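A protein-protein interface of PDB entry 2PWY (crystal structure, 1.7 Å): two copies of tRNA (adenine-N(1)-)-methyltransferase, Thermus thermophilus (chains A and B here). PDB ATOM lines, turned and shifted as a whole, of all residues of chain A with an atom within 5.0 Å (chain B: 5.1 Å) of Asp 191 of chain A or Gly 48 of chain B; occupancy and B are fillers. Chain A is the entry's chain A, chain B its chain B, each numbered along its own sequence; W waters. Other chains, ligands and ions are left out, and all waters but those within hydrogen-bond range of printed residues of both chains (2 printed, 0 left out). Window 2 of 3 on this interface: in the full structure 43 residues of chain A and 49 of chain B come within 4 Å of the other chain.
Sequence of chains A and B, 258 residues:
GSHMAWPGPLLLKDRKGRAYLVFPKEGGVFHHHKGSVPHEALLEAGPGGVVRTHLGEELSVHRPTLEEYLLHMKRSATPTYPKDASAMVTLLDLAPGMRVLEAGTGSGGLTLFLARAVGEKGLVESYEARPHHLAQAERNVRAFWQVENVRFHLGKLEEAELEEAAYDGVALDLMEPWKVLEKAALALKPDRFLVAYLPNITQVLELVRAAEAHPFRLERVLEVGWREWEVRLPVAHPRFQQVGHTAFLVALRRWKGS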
ATOM      1  N   LYS A 189      -0.338 -31.811  11.125  1.00  0.00           N
ATOM      2  CA  LYS A 189       0.984 -31.372  10.661  1.00  0.00           C
ATOM      3  C   LYS A 189       0.877 -30.572   9.371  1.00  0.00           C
ATOM      4  O   LYS A 189       0.085 -30.931   8.497  1.00  0.00           O
ATOM      5  CB  LYS A 189       1.881 -32.587  10.429  1.00  0.00           C
ATOM      6  CG  LYS A 189       2.348 -33.227  11.718  1.00  0.00           C
ATOM      7  CD  LYS A 189       3.120 -34.507  11.462  1.00  0.00           C
ATOM      8  CE  LYS A 189       3.443 -35.186  12.790  1.00  0.00           C
ATOM      9  NZ  LYS A 189       4.223 -36.423  12.538  1.00  0.00           N
ATOM     10  N   PRO A 190       1.661 -29.474   9.243  1.00  0.00           N
ATOM     11  CA  PRO A 190       1.758 -28.749   7.982  1.00  0.00           C
ATOM     12  C   PRO A 190       1.988 -29.675   6.783  1.00  0.00           C
ATOM     13  O   PRO A 190       2.795 -30.612   6.852  1.00  0.00           O
ATOM     14  CB  PRO A 190       2.968 -27.832   8.203  1.00  0.00           C
ATOM     15  CG  PRO A 190       2.890 -27.516   9.684  1.00  0.00           C
ATOM     16  CD  PRO A 190       2.461 -28.836  10.313  1.00  0.00           C
ATOM     17  N   ASP A 191       1.267 -29.395   5.698  1.00  0.00           N
ATOM     18  CA  ASP A 191       1.411 -30.076   4.408  1.00  0.00           C
ATOM     19  C   ASP A 191       0.740 -31.460   4.394  1.00  0.00           C
ATOM     20  O   ASP A 191       0.758 -32.141   3.378  1.00  0.00           O
ATOM     21  CB  ASP A 191       2.888 -30.171   3.984  1.00  0.00           C
ATOM     22  CG  ASP A 191       3.064 -30.005   2.491  1.00  0.00           C
ATOM     23  OD1 ASP A 191       2.323 -29.190   1.900  1.00  0.00           O
ATOM     24  OD2 ASP A 191       3.919 -30.695   1.905  1.00  0.00           O
ATOM     25  N   ARG A 192       0.131 -31.846   5.516  1.00  0.00           N
ATOM     26  CA  ARG A 192      -0.624 -33.096   5.594  1.00  0.00           C
ATOM     27  C   ARG A 192      -2.123 -32.838   5.382  1.00  0.00           C
ATOM     28  O   ARG A 192      -2.525 -31.695   5.159  1.00  0.00           O
ATOM     29  CB  ARG A 192      -0.308 -33.852   6.887  1.00  0.00           C
ATOM     30  CG  ARG A 192       1.186 -34.208   7.003  1.00  0.00           C
ATOM     31  CD  ARG A 192       1.601 -35.235   5.933  1.00  0.00           C
ATOM     32  NE  ARG A 192       0.933 -36.522   6.146  1.00  0.00           N
ATOM     33  CZ  ARG A 192       0.953 -37.554   5.306  1.00  0.00           C
ATOM     34  NH1 ARG A 192       1.603 -37.487   4.151  1.00  0.00           N
ATOM     35  NH2 ARG A 192       0.307 -38.670   5.633  1.00  0.00           N
ATOM     36  N   PHE A 193      -2.940 -33.894   5.396  1.00  0.00           N
ATOM     37  CA  PHE A 193      -4.299 -33.773   4.859  1.00  0.00           C
ATOM     38  C   PHE A 193      -5.405 -33.985   5.868  1.00  0.00           C
ATOM     39  O   PHE A 193      -5.260 -34.771   6.801  1.00  0.00           O
ATOM     40  CB  PHE A 193      -4.514 -34.747   3.693  1.00  0.00           C
ATOM     41  CG  PHE A 193      -3.600 -34.495   2.539  1.00  0.00           C
ATOM     42  CD1 PHE A 193      -3.960 -33.599   1.534  1.00  0.00           C
ATOM     43  CD2 PHE A 193      -2.351 -35.115   2.485  1.00  0.00           C
ATOM     44  CE1 PHE A 193      -3.098 -33.354   0.473  1.00  0.00           C
ATOM     45  CE2 PHE A 193      -1.491 -34.877   1.442  1.00  0.00           C
ATOM     46  CZ  PHE A 193      -1.866 -33.989   0.429  1.00  0.00           C
ATOM     47  N   ARG A 253      -5.384 -29.570   2.301  1.00  0.00           N
ATOM     48  CA  ARG A 253      -3.995 -29.661   2.757  1.00  0.00           C
ATOM     49  C   ARG A 253      -3.710 -28.547   3.745  1.00  0.00           C
ATOM     50  O   ARG A 253      -4.024 -27.382   3.470  1.00  0.00           O
ATOM     51  CB  ARG A 253      -3.019 -29.581   1.581  1.00  0.00           C
ATOM     52  CG  ARG A 253      -1.584 -29.950   1.938  1.00  0.00           C
ATOM     53  CD  ARG A 253      -0.616 -29.549   0.834  1.00  0.00           C
ATOM     54  NE  ARG A 253      -0.678 -30.361  -0.385  1.00  0.00           N
ATOM     55  CZ  ARG A 253       0.082 -31.426  -0.638  1.00  0.00           C
ATOM     56  NH1 ARG A 253       0.936 -31.885   0.262  1.00  0.00           N
ATOM     57  NH2 ARG A 253      -0.049 -32.059  -1.797  1.00  0.00           N
ATOM     58  N   ARG A 254      -3.116 -28.912   4.883  1.00  0.00           N
ATOM     59  CA  ARG A 254      -2.721 -27.972   5.939  1.00  0.00           C
ATOM     60  C   ARG A 254      -1.627 -27.042   5.429  1.00  0.00           C
ATOM     61  O   ARG A 254      -0.637 -27.497   4.854  1.00  0.00           O
ATOM     62  CB  ARG A 254      -2.216 -28.752   7.166  1.00  0.00           C
ATOM     63  CG  ARG A 254      -1.756 -27.911   8.386  1.00  0.00           C
ATOM     64  CD  ARG A 254      -2.892 -27.050   8.916  1.00  0.00           C
ATOM     65  NE  ARG A 254      -2.631 -26.361  10.194  1.00  0.00           N
ATOM     66  CZ  ARG A 254      -1.881 -25.265  10.356  1.00  0.00           C
ATOM     67  NH1 ARG A 254      -1.209 -24.728   9.349  1.00  0.00           N
ATOM     68  NH2 ARG A 254      -1.783 -24.705  11.557  1.00  0.00           N
ATOM     69  N   TRP A 255      -1.816 -25.745   5.640  1.00  0.00           N
ATOM     70  CA  TRP A 255      -0.817 -24.738   5.278  1.00  0.00           C
ATOM     71  C   TRP A 255       0.527 -24.999   5.930  1.00  0.00           C
ATOM     72  O   TRP A 255       0.590 -25.565   7.028  1.00  0.00           O
ATOM     73  CB  TRP A 255      -1.304 -23.365   5.728  1.00  0.00           C
ATOM     74  CG  TRP A 255      -2.297 -22.713   4.821  1.00  0.00           C
ATOM     75  CD1 TRP A 255      -2.933 -23.264   3.731  1.00  0.00           C
ATOM     76  CD2 TRP A 255      -2.806 -21.381   4.948  1.00  0.00           C
ATOM     77  NE1 TRP A 255      -3.790 -22.344   3.171  1.00  0.00           N
ATOM     78  CE2 TRP A 255      -3.732 -21.185   3.902  1.00  0.00           C
ATOM     79  CE3 TRP A 255      -2.571 -20.333   5.851  1.00  0.00           C
ATOM     80  CZ2 TRP A 255      -4.414 -19.973   3.726  1.00  0.00           C
ATOM     81  CZ3 TRP A 255      -3.257 -19.133   5.675  1.00  0.00           C
ATOM     82  CH2 TRP A 255      -4.163 -18.968   4.624  1.00  0.00           C
ATOM     83  N   LYS A 256       1.592 -24.574   5.238  1.00  0.00           N
ATOM     84  CA  LYS A 256       2.929 -24.431   5.810  1.00  0.00           C
ATOM     85  C   LYS A 256       2.849 -23.850   7.216  1.00  0.00           C
ATOM     86  O   LYS A 256       2.072 -22.914   7.477  1.00  0.00           O
ATOM     87  CB  LYS A 256       3.776 -23.496   4.928  1.00  0.00           C
ATOM     88  CG  LYS A 256       5.230 -23.350   5.354  1.00  0.00           C
ATOM     89  CD  LYS A 256       5.948 -22.291   4.495  1.00  0.00           C
ATOM     90  CE  LYS A 256       7.450 -22.294   4.741  1.00  0.00           C
ATOM     91  NZ  LYS A 256       7.749 -22.028   6.160  1.00  0.00           N
ATOM     92  N   GLY B  46      11.163 -26.289   3.324  1.00  0.00           N
ATOM     93  CA  GLY B  46      10.251 -26.903   4.291  1.00  0.00           C
ATOM     94  C   GLY B  46       8.965 -27.418   3.654  1.00  0.00           C
ATOM     95  O   GLY B  46       8.691 -27.134   2.483  1.00  0.00           O
ATOM     96  N   PRO B  47       8.153 -28.169   4.432  1.00  0.00           N
ATOM     97  CA  PRO B  47       6.915 -28.749   3.903  1.00  0.00           C
ATOM     98  C   PRO B  47       5.857 -27.674   3.616  1.00  0.00           C
ATOM     99  O   PRO B  47       5.440 -26.948   4.525  1.00  0.00           O
ATOM    100  CB  PRO B  47       6.445 -29.690   5.025  1.00  0.00           C
ATOM    101  CG  PRO B  47       7.576 -29.763   6.022  1.00  0.00           C
ATOM    102  CD  PRO B  47       8.355 -28.500   5.855  1.00  0.00           C
ATOM    103  N   GLY B  48       5.440 -27.583   2.355  1.00  0.00           N
ATOM    104  CA  GLY B  48       4.446 -26.601   1.941  1.00  0.00           C
ATOM    105  C   GLY B  48       5.047 -25.234   1.646  1.00  0.00           C
ATOM    106  O   GLY B  48       4.316 -24.265   1.455  1.00  0.00           O
ATOM    107  N   GLY B  49       6.377 -25.161   1.609  1.00  0.00           N
ATOM    108  CA  GLY B  49       7.073 -23.912   1.296  1.00  0.00           C
ATOM    109  C   GLY B  49       7.082 -23.667  -0.196  1.00  0.00           C
ATOM    110  O   GLY B  49       6.815 -24.586  -0.981  1.00  0.00           O
ATOM    111  N   VAL B  50       7.394 -22.434  -0.603  1.00  0.00           N
ATOM    112  CA  VAL B  50       7.486 -22.125  -2.033  1.00  0.00           C
ATOM    113  C   VAL B  50       8.868 -21.648  -2.446  1.00  0.00           C
ATOM    114  O   VAL B  50       9.583 -21.002  -1.669  1.00  0.00           O
ATOM    115  CB  VAL B  50       6.417 -21.095  -2.532  1.00  0.00           C
ATOM    116  CG1 VAL B  50       5.052 -21.746  -2.621  1.00  0.00           C
ATOM    117  CG2 VAL B  50       6.376 -19.854  -1.653  1.00  0.00           C
ATOM    118  N   VAL B  61       6.729 -26.889  -2.476  1.00  0.00           N
ATOM    119  CA  VAL B  61       7.637 -27.977  -2.108  1.00  0.00           C
ATOM    120  C   VAL B  61       6.951 -28.925  -1.112  1.00  0.00           C
ATOM    121  O   VAL B  61       6.360 -28.486  -0.117  1.00  0.00           O
ATOM    122  CB  VAL B  61       8.957 -27.422  -1.524  1.00  0.00           C
ATOM    123  CG1 VAL B  61       9.950 -28.544  -1.255  1.00  0.00           C
ATOM    124  CG2 VAL B  61       9.584 -26.385  -2.482  1.00  0.00           C
ATOM    125  N   HIS B  62       7.023 -30.225  -1.393  1.00  0.00           N
ATOM    126  CA  HIS B  62       6.274 -31.231  -0.632  1.00  0.00           C
ATOM    127  C   HIS B  62       7.070 -32.515  -0.496  1.00  0.00           C
ATOM    128  O   HIS B  62       7.933 -32.802  -1.330  1.00  0.00           O
ATOM    129  CB  HIS B  62       4.951 -31.561  -1.334  1.00  0.00           C
ATOM    130  CG  HIS B  62       4.116 -30.362  -1.654  1.00  0.00           C
ATOM    131  ND1 HIS B  62       3.305 -29.747  -0.725  1.00  0.00           N
ATOM    132  CD2 HIS B  62       3.969 -29.662  -2.804  1.00  0.00           C
ATOM    133  CE1 HIS B  62       2.694 -28.719  -1.289  1.00  0.00           C
ATOM    134  NE2 HIS B  62       3.081 -28.645  -2.550  1.00  0.00           N
ATOM    135  N   ARG B  63       6.795 -33.279   0.562  1.00  0.00           N
ATOM    136  CA  ARG B  63       7.164 -34.683   0.572  1.00  0.00           C
ATOM    137  C   ARG B  63       5.995 -35.367  -0.140  1.00  0.00           C
ATOM    138  O   ARG B  63       4.837 -35.142   0.229  1.00  0.00           O
ATOM    139  CB  ARG B  63       7.363 -35.207   1.996  1.00  0.00           C
HETATM  140  O   HOH W   1       5.202 -32.762   2.599  1.00  0.00           O
HETATM  141  O   HOH W   2       2.458 -33.983  -0.784  1.00  0.00           O
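Among the printed residues, merely in contact across the chains: Lys 256 of chain A with Gly 48 of chain B (3.6 Å), Lys 256 of chain A with Pro 47 of chain B (3.7 Å), Asp 191 of chain A with Pro 47 of chain B (3.7 Å), Lys 256 of chain A with Gly 49 of chain B (3.8 Å) and Asp 191 of chain A with Val 61 of chain B (3.9 Å).
The side-chain carboxylate (OD1) of Asp 191 of chain A lies within salt-bridge range of the guanidinium group (NH1) of Arg 253 of chain A, 3.4 Å away. O of Arg 254 of chain A is in hydrogen-bond range of N of Asp 191 of chain A. The backbone NH (N) of Gly 48 of chain B is in hydrogen-bond range of the backbone carbonyl oxygen (O) of Val 61 of chain B. The backbone carbonyl oxygen of Gly 49 of chain B sits at hydrogen-bond distance from the backbone NH of Val 61 of chain B (2.7 Å).
Water W1 lies within hydrogen-bond range of the side-chain carboxylate (OD2) of Asp 191 of chain A and the backbone NH (N) of Arg 63 of chain B. Water W2 bridges the guanidinium group of Arg 253 of chain A (2.8 Å) and the backbone carbonyl oxygen of Arg 63 of chain B (2.8 Å).
The backbone NH (N) of Gly 48 of chain B sits close to the side-chain carboxylate (OD2) of Asp 191 of chain A (3.5 Å). The side-chain carboxylate (OD1) of Asp 191 of chain A is in hydrogen-bond range of a ring nitrogen (ND1) of His 62 of chain B (2.9 Å). The guanidinium group (NH1) of Arg 253 of chain A sits at hydrogen-bond distance from a ring nitrogen (ND1) of His 62 of chain B, at 3.3 Å.
Asp 191 of chain A touches just these residues of chain B: Pro 47 (3.7 Å), Gly 48 (3.3 Å), Val 61 (3.9 Å) and His 62 (2.9 Å). Of chain A, only Asp 191 (3.3 Å) and Lys 256 (3.6 Å) come within 4 Å of Gly 48 of chain B. Printed residues of chain B within 4 Å of Lys 256 of chain A: Pro 47 (3.7 Å), Gly 48 (3.6 Å) and Gly 49 (3.8 Å). Printed residues of chain A within 4 Å of Pro 47 of chain B: Asp 191 (3.7 Å) and Lys 256 (3.7 Å). Of the printed residues of chain A, Gly 49 of chain B touches Lys 256 (3.8 Å). Of the printed residues of chain A, His 62 of chain B touches Asp 191 and Arg 253. Printed residues of chain B within 4 Å of Arg 253 of chain A: His 62 (3.3 Å). The nearest residue of chain B that does not touch Asp 191 of chain A is Arg 63 of chain B (4.1 Å). The nearest printed residue of chain A that does not touch Gly 48 of chain B is Trp 255 of chain A (5.8 Å). The nearest printed residue of chain B that does not touch Lys 256 of chain A is Val 50 of chain B (5.3 Å).
Printed residues of chain A that touch a printed residue of chain B: Asp 191, Arg 253 and Lys 256. Of the 8 printed residues of chain B, 5 touch a printed residue of chain A. Hydrophobic or aromatic side chains of chain B within 4 Å of the printed part of chain A: Pro 47 and His 62. Among the printed residues, no Asp or Glu carboxylate lies within 4 Å of a Lys or Arg side-chain nitrogen of the other chain.
No position is printed for both chains. Of the 8 pairs that touch across the chains among the printed residues, none has its exchanged pair printed and touching as well.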
